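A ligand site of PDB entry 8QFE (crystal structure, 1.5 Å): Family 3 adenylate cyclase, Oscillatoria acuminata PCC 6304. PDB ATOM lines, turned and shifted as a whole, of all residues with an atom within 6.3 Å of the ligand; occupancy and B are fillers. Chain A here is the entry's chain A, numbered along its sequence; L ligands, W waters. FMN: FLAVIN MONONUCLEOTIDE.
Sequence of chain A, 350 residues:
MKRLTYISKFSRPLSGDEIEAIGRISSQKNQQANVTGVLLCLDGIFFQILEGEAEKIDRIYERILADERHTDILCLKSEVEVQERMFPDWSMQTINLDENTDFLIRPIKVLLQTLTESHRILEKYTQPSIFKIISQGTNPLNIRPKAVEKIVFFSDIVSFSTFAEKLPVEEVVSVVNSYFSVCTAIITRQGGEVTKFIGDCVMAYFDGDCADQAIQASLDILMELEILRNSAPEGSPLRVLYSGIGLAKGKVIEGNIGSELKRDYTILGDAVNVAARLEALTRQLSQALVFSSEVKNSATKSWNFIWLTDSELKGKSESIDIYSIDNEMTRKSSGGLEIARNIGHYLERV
O of Ile 64 sits at hydrogen-bond distance from NE2 of His 70, 2.9 Å away.
The guanidinium group of Arg 69 lies within salt-bridge range of the side-chain carboxylate of Asp 67 (2.8 Å).
OD1 of Asn 30 lies close to O of Ser 26.
N of Phe 46 sits at hydrogen-bond distance from O of Ser 8 (2.9 Å).
NE2 of Gln 48 sits close to SD of Met 92, at 3.5 Å.
The side-chain amide oxygen (OE1) of Gln 48 lies within hydrogen-bond range of the side-chain hydroxyl (OH) of Tyr 6, at 2.7 Å.
ND1 of His 70 is in hydrogen-bond range of OG of Ser 8.
OG of Ser 26 is in hydrogen-bond range of O of Ile 22 (2.8 Å).
Water W2 bridges O3P of the ligand and NH2 of Arg 63.
Water W4 lies within hydrogen-bond range of the side-chain amide oxygen of Asn 30 and an oxygen (O2) of the ligand.
Water W3 bridges NH2 of Arg 69 (2.8 Å) and O3' of the ligand (3.4 Å).
Merely in contact with the ligand: Tyr 6 (3.5 Å), Ile 22 (3.7 Å), Leu 39 (3.9 Å), Phe 46 (3.6 Å), Leu 50 (3.2 Å), Ile 60 (3.8 Å), Arg 63 (3.7 Å), Ile 64 (3.5 Å), His 70 (3.8 Å) and Met 92 (3.8 Å).
The nearest printed residue that does not touch the ligand is Ile 25 (4.1 Å).
A nitrogen (N3) of the ligand sits at hydrogen-bond distance from the side-chain amide oxygen (OD1) of Asn 30 (2.9 Å).
NH2 of Arg 69 lies within hydrogen-bond range of O3' of the ligand, 3.5 Å away.
NZ of Lys 29 is in hydrogen-bond range of O4' of the ligand (2.7 Å).
A nitrogen (N5) of the ligand lies close to the side-chain hydroxyl of Ser 26, at 3.3 Å.
The side-chain carboxylate of Asp 67 sits at hydrogen-bond distance from an oxygen (O2') of the ligand, at 2.9 Å.
The side-chain amide nitrogen (NE2) of Gln 48 sits at hydrogen-bond distance from a nitrogen (N5) of the ligand.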
ATOM      1  N   TYR A   6     -30.612 -10.465  23.811  1.00  0.00           N
ATOM      2  CA  TYR A   6     -31.284  -9.974  25.027  1.00  0.00           C
ATOM      3  C   TYR A   6     -30.836  -8.567  25.366  1.00  0.00           C
ATOM      4  O   TYR A   6     -29.838  -8.068  24.814  1.00  0.00           O
ATOM      5  CB  TYR A   6     -31.050 -10.929  26.238  1.00  0.00           C
ATOM      6  CG  TYR A   6     -29.674 -10.819  26.842  1.00  0.00           C
ATOM      7  CD1 TYR A   6     -29.394  -9.833  27.744  1.00  0.00           C
ATOM      8  CD2 TYR A   6     -28.654 -11.687  26.444  1.00  0.00           C
ATOM      9  CE1 TYR A   6     -28.112  -9.695  28.292  1.00  0.00           C
ATOM     10  CE2 TYR A   6     -27.387 -11.575  26.996  1.00  0.00           C
ATOM     11  CZ  TYR A   6     -27.110 -10.546  27.891  1.00  0.00           C
ATOM     12  OH  TYR A   6     -25.836 -10.367  28.419  1.00  0.00           O
ATOM     13  N   SER A   8     -30.515  -5.892  28.957  1.00  0.00           N
ATOM     14  CA  SER A   8     -30.540  -5.844  30.407  1.00  0.00           C
ATOM     15  C   SER A   8     -30.202  -4.450  30.905  1.00  0.00           C
ATOM     16  O   SER A   8     -29.737  -3.599  30.138  1.00  0.00           O
ATOM     17  CB  SER A   8     -29.562  -6.867  31.023  1.00  0.00           C
ATOM     18  OG  SER A   8     -28.181  -6.464  30.738  1.00  0.00           O
ATOM     19  N   LEU A  14     -21.309   1.220  36.235  1.00  0.00           N
ATOM     20  CA  LEU A  14     -20.133   0.500  35.741  1.00  0.00           C
ATOM     21  C   LEU A  14     -19.278   1.447  34.904  1.00  0.00           C
ATOM     22  O   LEU A  14     -19.788   2.142  34.036  1.00  0.00           O
ATOM     23  CB  LEU A  14     -20.577  -0.690  34.894  1.00  0.00           C
ATOM     24  CG  LEU A  14     -21.436  -1.769  35.552  1.00  0.00           C
ATOM     25  CD1 LEU A  14     -21.961  -2.772  34.548  1.00  0.00           C
ATOM     26  CD2 LEU A  14     -20.619  -2.481  36.644  1.00  0.00           C
ATOM     27  N   ILE A  22     -15.451  -7.029  31.216  1.00  0.00           N
ATOM     28  CA  ILE A  22     -16.443  -8.043  30.882  1.00  0.00           C
ATOM     29  C   ILE A  22     -16.195  -8.577  29.478  1.00  0.00           C
ATOM     30  O   ILE A  22     -16.189  -9.791  29.234  1.00  0.00           O
ATOM     31  CB  ILE A  22     -17.865  -7.458  31.043  1.00  0.00           C
ATOM     32  CG1 ILE A  22     -18.162  -7.169  32.503  1.00  0.00           C
ATOM     33  CG2 ILE A  22     -18.905  -8.409  30.424  1.00  0.00           C
ATOM     34  CD1 ILE A  22     -19.411  -6.317  32.743  1.00  0.00           C
ATOM     35  N   ILE A  25     -13.107 -11.051  29.303  1.00  0.00           N
ATOM     36  CA  ILE A  25     -13.396 -12.367  29.857  1.00  0.00           C
ATOM     37  C   ILE A  25     -14.371 -13.129  28.946  1.00  0.00           C
ATOM     38  O   ILE A  25     -14.170 -14.328  28.662  1.00  0.00           O
ATOM     39  CB  ILE A  25     -13.930 -12.234  31.302  1.00  0.00           C
ATOM     40  CG1 ILE A  25     -12.793 -11.765  32.210  1.00  0.00           C
ATOM     41  CG2 ILE A  25     -14.516 -13.529  31.762  1.00  0.00           C
ATOM     42  CD1 ILE A  25     -13.247 -11.390  33.633  1.00  0.00           C
ATOM     43  N   SER A  26     -15.385 -12.426  28.420  1.00  0.00           N
ATOM     44  CA  SER A  26     -16.326 -13.061  27.499  1.00  0.00           C
ATOM     45  C   SER A  26     -15.618 -13.574  26.255  1.00  0.00           C
ATOM     46  O   SER A  26     -15.908 -14.673  25.786  1.00  0.00           O
ATOM     47  CB  SER A  26     -17.437 -12.053  27.084  1.00  0.00           C
ATOM     48  OG  SER A  26     -18.094 -11.620  28.257  1.00  0.00           O
ATOM     49  N   SER A  27     -14.697 -12.786  25.713  1.00  0.00           N
ATOM     50  CA  SER A  27     -14.002 -13.212  24.505  1.00  0.00           C
ATOM     51  C   SER A  27     -13.111 -14.415  24.785  1.00  0.00           C
ATOM     52  O   SER A  27     -13.053 -15.344  23.981  1.00  0.00           O
ATOM     53  CB  SER A  27     -13.176 -12.047  23.956  1.00  0.00           C
ATOM     54  OG  SER A  27     -12.593 -12.402  22.724  1.00  0.00           O
ATOM     55  N   LYS A  29     -13.499 -16.780  27.086  1.00  0.00           N
ATOM     56  CA  LYS A  29     -14.284 -17.979  27.279  1.00  0.00           C
ATOM     57  C   LYS A  29     -15.015 -18.397  26.000  1.00  0.00           C
ATOM     58  O   LYS A  29     -15.014 -19.583  25.650  1.00  0.00           O
ATOM     59  CB  LYS A  29     -15.282 -17.754  28.409  1.00  0.00           C
ATOM     60  CG  LYS A  29     -14.623 -17.573  29.770  1.00  0.00           C
ATOM     61  CD  LYS A  29     -15.600 -17.378  30.905  1.00  0.00           C
ATOM     62  CE  LYS A  29     -16.480 -18.601  31.148  1.00  0.00           C
ATOM     63  NZ  LYS A  29     -17.271 -18.405  32.417  1.00  0.00           N
ATOM     64  N   ASN A  30     -15.599 -17.432  25.271  1.00  0.00           N
ATOM     65  CA  ASN A  30     -16.370 -17.794  24.096  1.00  0.00           C
ATOM     66  C   ASN A  30     -15.490 -18.403  23.003  1.00  0.00           C
ATOM     67  O   ASN A  30     -15.920 -19.308  22.292  1.00  0.00           O
ATOM     68  CB  ASN A  30     -17.111 -16.566  23.564  1.00  0.00           C
ATOM     69  CG  ASN A  30     -18.267 -16.138  24.442  1.00  0.00           C
ATOM     70  OD1 ASN A  30     -18.607 -16.791  25.428  1.00  0.00           O
ATOM     71  ND2 ASN A  30     -18.886 -15.006  24.055  1.00  0.00           N
ATOM     72  N   VAL A  35     -18.182 -19.957  20.435  1.00  0.00           N
ATOM     73  CA  VAL A  35     -19.308 -19.024  20.505  1.00  0.00           C
ATOM     74  C   VAL A  35     -18.827 -17.672  20.003  1.00  0.00           C
ATOM     75  O   VAL A  35     -17.669 -17.280  20.256  1.00  0.00           O
ATOM     76  CB  VAL A  35     -19.830 -18.931  21.952  1.00  0.00           C
ATOM     77  CG1 VAL A  35     -20.775 -17.746  22.155  1.00  0.00           C
ATOM     78  CG2 VAL A  35     -20.514 -20.243  22.351  1.00  0.00           C
ATOM     79  N   LEU A  39     -21.527  -7.380  22.080  1.00  0.00           N
ATOM     80  CA  LEU A  39     -21.994  -6.806  23.349  1.00  0.00           C
ATOM     81  C   LEU A  39     -21.922  -5.286  23.223  1.00  0.00           C
ATOM     82  O   LEU A  39     -20.835  -4.718  23.005  1.00  0.00           O
ATOM     83  CB  LEU A  39     -21.143  -7.297  24.523  1.00  0.00           C
ATOM     84  CG  LEU A  39     -21.475  -6.636  25.869  1.00  0.00           C
ATOM     85  CD1 LEU A  39     -22.891  -6.932  26.357  1.00  0.00           C
ATOM     86  CD2 LEU A  39     -20.447  -7.060  26.970  1.00  0.00           C
ATOM     87  N   PHE A  46     -27.358  -2.847  28.615  1.00  0.00           N
ATOM     88  CA  PHE A  46     -26.623  -3.802  27.789  1.00  0.00           C
ATOM     89  C   PHE A  46     -27.520  -4.412  26.723  1.00  0.00           C
ATOM     90  O   PHE A  46     -28.713  -4.643  26.939  1.00  0.00           O
ATOM     91  CB  PHE A  46     -26.054  -4.962  28.620  1.00  0.00           C
ATOM     92  CG  PHE A  46     -24.891  -4.651  29.484  1.00  0.00           C
ATOM     93  CD1 PHE A  46     -23.695  -4.222  28.923  1.00  0.00           C
ATOM     94  CD2 PHE A  46     -24.959  -4.826  30.857  1.00  0.00           C
ATOM     95  CE1 PHE A  46     -22.570  -3.990  29.766  1.00  0.00           C
ATOM     96  CE2 PHE A  46     -23.831  -4.594  31.682  1.00  0.00           C
ATOM     97  CZ  PHE A  46     -22.653  -4.178  31.125  1.00  0.00           C
ATOM     98  N   GLN A  48     -26.937  -7.750  23.950  1.00  0.00           N
ATOM     99  CA  GLN A  48     -25.999  -8.809  23.573  1.00  0.00           C
ATOM    100  C   GLN A  48     -26.637  -9.775  22.591  1.00  0.00           C
ATOM    101  O   GLN A  48     -27.816 -10.168  22.738  1.00  0.00           O
ATOM    102  CB  GLN A  48     -25.462  -9.583  24.787  1.00  0.00           C
ATOM    103  CG  GLN A  48     -24.293 -10.548  24.409  1.00  0.00           C
ATOM    104  CD  GLN A  48     -23.538 -11.099  25.634  1.00  0.00           C
ATOM    105  OE1 GLN A  48     -24.149 -11.411  26.592  1.00  0.00           O
ATOM    106  NE2 GLN A  48     -22.245 -11.237  25.547  1.00  0.00           N
ATOM    107  N   LEU A  50     -25.479 -13.664  21.144  1.00  0.00           N
ATOM    108  CA  LEU A  50     -24.628 -14.831  21.364  1.00  0.00           C
ATOM    109  C   LEU A  50     -25.052 -15.914  20.384  1.00  0.00           C
ATOM    110  O   LEU A  50     -26.256 -16.145  20.207  1.00  0.00           O
ATOM    111  CB  LEU A  50     -24.757 -15.358  22.789  1.00  0.00           C
ATOM    112  CG  LEU A  50     -24.227 -14.479  23.897  1.00  0.00           C
ATOM    113  CD1 LEU A  50     -24.894 -14.824  25.239  1.00  0.00           C
ATOM    114  CD2 LEU A  50     -22.723 -14.617  24.012  1.00  0.00           C
ATOM    115  N   ILE A  60     -23.976 -20.869  28.957  1.00  0.00           N
ATOM    116  CA  ILE A  60     -23.440 -19.506  29.048  1.00  0.00           C
ATOM    117  C   ILE A  60     -24.524 -18.535  29.503  1.00  0.00           C
ATOM    118  O   ILE A  60     -24.292 -17.696  30.378  1.00  0.00           O
ATOM    119  CB  ILE A  60     -22.823 -19.073  27.696  1.00  0.00           C
ATOM    120  CG1 ILE A  60     -21.575 -19.912  27.438  1.00  0.00           C
ATOM    121  CG2 ILE A  60     -22.528 -17.607  27.706  1.00  0.00           C
ATOM    122  CD1 ILE A  60     -21.142 -19.847  25.961  1.00  0.00           C
ATOM    123  N   ARG A  63     -25.238 -18.691  33.154  1.00  0.00           N
ATOM    124  CA  ARG A  63     -24.202 -18.010  33.925  1.00  0.00           C
ATOM    125  C   ARG A  63     -24.416 -16.499  33.866  1.00  0.00           C
ATOM    126  O   ARG A  63     -24.241 -15.800  34.875  1.00  0.00           O
ATOM    127  CB  ARG A  63     -22.807 -18.390  33.433  1.00  0.00           C
ATOM    128  CG  ARG A  63     -21.663 -17.779  34.246  1.00  0.00           C
ATOM    129  CD  ARG A  63     -21.650 -18.249  35.703  1.00  0.00           C
ATOM    130  NE  ARG A  63     -20.662 -17.535  36.506  1.00  0.00           N
ATOM    131  CZ  ARG A  63     -20.823 -16.311  36.989  1.00  0.00           C
ATOM    132  NH1 ARG A  63     -21.948 -15.610  36.778  1.00  0.00           N
ATOM    133  NH2 ARG A  63     -19.824 -15.763  37.693  1.00  0.00           N
ATOM    134  N   ILE A  64     -24.750 -15.982  32.679  1.00  0.00           N
ATOM    135  CA  ILE A  64     -24.982 -14.541  32.531  1.00  0.00           C
ATOM    136  C   ILE A  64     -26.167 -14.114  33.399  1.00  0.00           C
ATOM    137  O   ILE A  64     -26.147 -13.051  34.019  1.00  0.00           O
ATOM    138  CB  ILE A  64     -25.184 -14.183  31.058  1.00  0.00           C
ATOM    139  CG1 ILE A  64     -23.877 -14.394  30.280  1.00  0.00           C
ATOM    140  CG2 ILE A  64     -25.721 -12.763  30.892  1.00  0.00           C
ATOM    141  CD1 ILE A  64     -24.063 -14.297  28.804  1.00  0.00           C
ATOM    142  N   LEU A  65     -27.177 -14.983  33.537  1.00  0.00           N
ATOM    143  CA  LEU A  65     -28.322 -14.637  34.355  1.00  0.00           C
ATOM    144  C   LEU A  65     -27.956 -14.514  35.835  1.00  0.00           C
ATOM    145  O   LEU A  65     -28.697 -13.881  36.610  1.00  0.00           O
ATOM    146  CB  LEU A  65     -29.410 -15.688  34.193  1.00  0.00           C
ATOM    147  CG  LEU A  65     -30.234 -15.746  32.949  1.00  0.00           C
ATOM    148  CD1 LEU A  65     -31.208 -16.913  32.996  1.00  0.00           C
ATOM    149  CD2 LEU A  65     -31.039 -14.461  32.763  1.00  0.00           C
ATOM    150  N   ALA A  66     -26.872 -15.175  36.272  1.00  0.00           N
ATOM    151  CA  ALA A  66     -26.381 -15.098  37.639  1.00  0.00           C
ATOM    152  C   ALA A  66     -25.450 -13.908  37.896  1.00  0.00           C
ATOM    153  O   ALA A  66     -25.026 -13.719  39.033  1.00  0.00           O
ATOM    154  CB  ALA A  66     -25.671 -16.400  37.969  1.00  0.00           C
ATOM    155  N   ASP A  67     -25.084 -13.139  36.882  1.00  0.00           N
ATOM    156  CA  ASP A  67     -24.153 -12.033  37.099  1.00  0.00           C
ATOM    157  C   ASP A  67     -24.839 -10.874  37.805  1.00  0.00           C
ATOM    158  O   ASP A  67     -25.809 -10.304  37.300  1.00  0.00           O
ATOM    159  CB  ASP A  67     -23.597 -11.572  35.754  1.00  0.00           C
ATOM    160  CG  ASP A  67     -22.313 -10.771  35.865  1.00  0.00           C
ATOM    161  OD1 ASP A  67     -21.312 -11.181  35.249  1.00  0.00           O
ATOM    162  OD2 ASP A  67     -22.336  -9.740  36.608  1.00  0.00           O
ATOM    163  N   ARG A  69     -24.022  -7.859  38.098  1.00  0.00           N
ATOM    164  CA  ARG A  69     -23.819  -6.516  37.524  1.00  0.00           C
ATOM    165  C   ARG A  69     -24.933  -6.052  36.608  1.00  0.00           C
ATOM    166  O   ARG A  69     -24.925  -4.883  36.241  1.00  0.00           O
ATOM    167  CB  ARG A  69     -22.511  -6.483  36.751  1.00  0.00           C
ATOM    168  CG  ARG A  69     -21.312  -6.625  37.737  1.00  0.00           C
ATOM    169  CD  ARG A  69     -20.019  -6.858  37.010  1.00  0.00           C
ATOM    170  NE  ARG A  69     -19.924  -8.169  36.385  1.00  0.00           N
ATOM    171  CZ  ARG A  69     -18.815  -8.674  35.863  1.00  0.00           C
ATOM    172  NH1 ARG A  69     -17.678  -7.987  35.884  1.00  0.00           N
ATOM    173  NH2 ARG A  69     -18.826  -9.884  35.324  1.00  0.00           N
ATOM    174  N   HIS A  70     -25.883  -6.916  36.247  1.00  0.00           N
ATOM    175  CA  HIS A  70     -27.058  -6.494  35.503  1.00  0.00           C
ATOM    176  C   HIS A  70     -28.300  -7.184  36.074  1.00  0.00           C
ATOM    177  O   HIS A  70     -28.237  -8.134  36.897  1.00  0.00           O
ATOM    178  CB  HIS A  70     -26.859  -6.681  33.990  1.00  0.00           C
ATOM    179  CG  HIS A  70     -26.691  -8.080  33.507  1.00  0.00           C
ATOM    180  ND1 HIS A  70     -26.743  -8.393  32.162  1.00  0.00           N
ATOM    181  CD2 HIS A  70     -26.457  -9.251  34.157  1.00  0.00           C
ATOM    182  CE1 HIS A  70     -26.570  -9.701  32.017  1.00  0.00           C
ATOM    183  NE2 HIS A  70     -26.421 -10.239  33.217  1.00  0.00           N
ATOM    184  N   SER A  91     -15.323 -13.364  18.860  1.00  0.00           N
ATOM    185  CA  SER A  91     -15.693 -14.222  19.981  1.00  0.00           C
ATOM    186  C   SER A  91     -16.624 -13.468  20.933  1.00  0.00           C
ATOM    187  O   SER A  91     -17.646 -14.015  21.418  1.00  0.00           O
ATOM    188  CB  SER A  91     -14.425 -14.642  20.704  1.00  0.00           C
ATOM    189  OG  SER A  91     -13.769 -15.645  19.925  1.00  0.00           O
ATOM    190  N   MET A  92     -16.271 -12.223  21.238  1.00  0.00           N
ATOM    191  CA  MET A  92     -17.264 -11.287  21.761  1.00  0.00           C
ATOM    192  C   MET A  92     -16.722  -9.871  21.537  1.00  0.00           C
ATOM    193  O   MET A  92     -15.871  -9.404  22.295  1.00  0.00           O
ATOM    194  CB  MET A  92     -17.588 -11.585  23.250  1.00  0.00           C
ATOM    195  CG  MET A  92     -18.497 -10.341  23.638  1.00  0.00           C
ATOM    196  SD  MET A  92     -20.166 -10.523  22.861  1.00  0.00           S
ATOM    197  CE  MET A  92     -20.590 -12.242  22.797  1.00  0.00           C
HETATM  198  N1  FMN L   1     -19.455 -14.693  30.090  1.00  0.00           N
HETATM  199  C2  FMN L   1     -19.136 -15.587  29.051  1.00  0.00           C
HETATM  200  O2  FMN L   1     -18.534 -16.566  29.280  1.00  0.00           O
HETATM  201  N3  FMN L   1     -19.557 -15.285  27.663  1.00  0.00           N
HETATM  202  C4  FMN L   1     -20.316 -14.094  27.410  1.00  0.00           C
HETATM  203  O4  FMN L   1     -20.624 -13.832  26.262  1.00  0.00           O
HETATM  204  C4A FMN L   1     -20.592 -13.212  28.525  1.00  0.00           C
HETATM  205  N5  FMN L   1     -21.388 -12.034  28.349  1.00  0.00           N
HETATM  206  C5A FMN L   1     -21.672 -11.150  29.428  1.00  0.00           C
HETATM  207  C6  FMN L   1     -22.502  -9.993  29.287  1.00  0.00           C
HETATM  208  C7  FMN L   1     -22.768  -9.184  30.366  1.00  0.00           C
HETATM  209  C7M FMN L   1     -23.626  -8.001  29.986  1.00  0.00           C
HETATM  210  C8  FMN L   1     -22.356  -9.496  31.665  1.00  0.00           C
HETATM  211  C8M FMN L   1     -22.720  -8.558  32.772  1.00  0.00           C
HETATM  212  C9  FMN L   1     -21.575 -10.636  31.809  1.00  0.00           C
HETATM  213  C9A FMN L   1     -21.271 -11.454  30.755  1.00  0.00           C
HETATM  214  N10 FMN L   1     -20.458 -12.679  30.941  1.00  0.00           N
HETATM  215  C10 FMN L   1     -20.223 -13.509  29.882  1.00  0.00           C
HETATM  216  C1' FMN L   1     -19.872 -13.021  32.251  1.00  0.00           C
HETATM  217  C2' FMN L   1     -20.441 -14.094  33.089  1.00  0.00           C
HETATM  218  O2' FMN L   1     -21.600 -13.538  33.584  1.00  0.00           O
HETATM  219  C3' FMN L   1     -19.389 -14.440  34.162  1.00  0.00           C
HETATM  220  O3' FMN L   1     -18.885 -13.339  34.863  1.00  0.00           O
HETATM  221  C4' FMN L   1     -18.181 -15.125  33.526  1.00  0.00           C
HETATM  222  O4' FMN L   1     -18.563 -16.055  32.566  1.00  0.00           O
HETATM  223  C5' FMN L   1     -17.404 -15.883  34.654  1.00  0.00           C
HETATM  224  O5' FMN L   1     -16.275 -16.404  34.031  1.00  0.00           O
HETATM  225  P   FMN L   1     -14.951 -16.762  35.001  1.00  0.00           P
HETATM  226  O1P FMN L   1     -13.833 -17.359  34.191  1.00  0.00           O
HETATM  227  O2P FMN L   1     -14.450 -15.517  35.674  1.00  0.00           O
HETATM  228  O3P FMN L   1     -15.572 -17.620  36.082  1.00  0.00           O
HETATM  229  O   HOH W   1     -12.693 -20.164  34.994  1.00  0.00           O
HETATM  230  O   HOH W   2     -16.969 -17.139  38.067  1.00  0.00           O
HETATM  231  O   HOH W   3     -16.587 -10.939  33.994  1.00  0.00           O
HETATM  232  O   HOH W   4     -18.320 -18.714  27.438  1.00  0.00           O
HETATM  233  O   HOH W   5     -14.559 -19.317  37.797  1.00  0.00           O
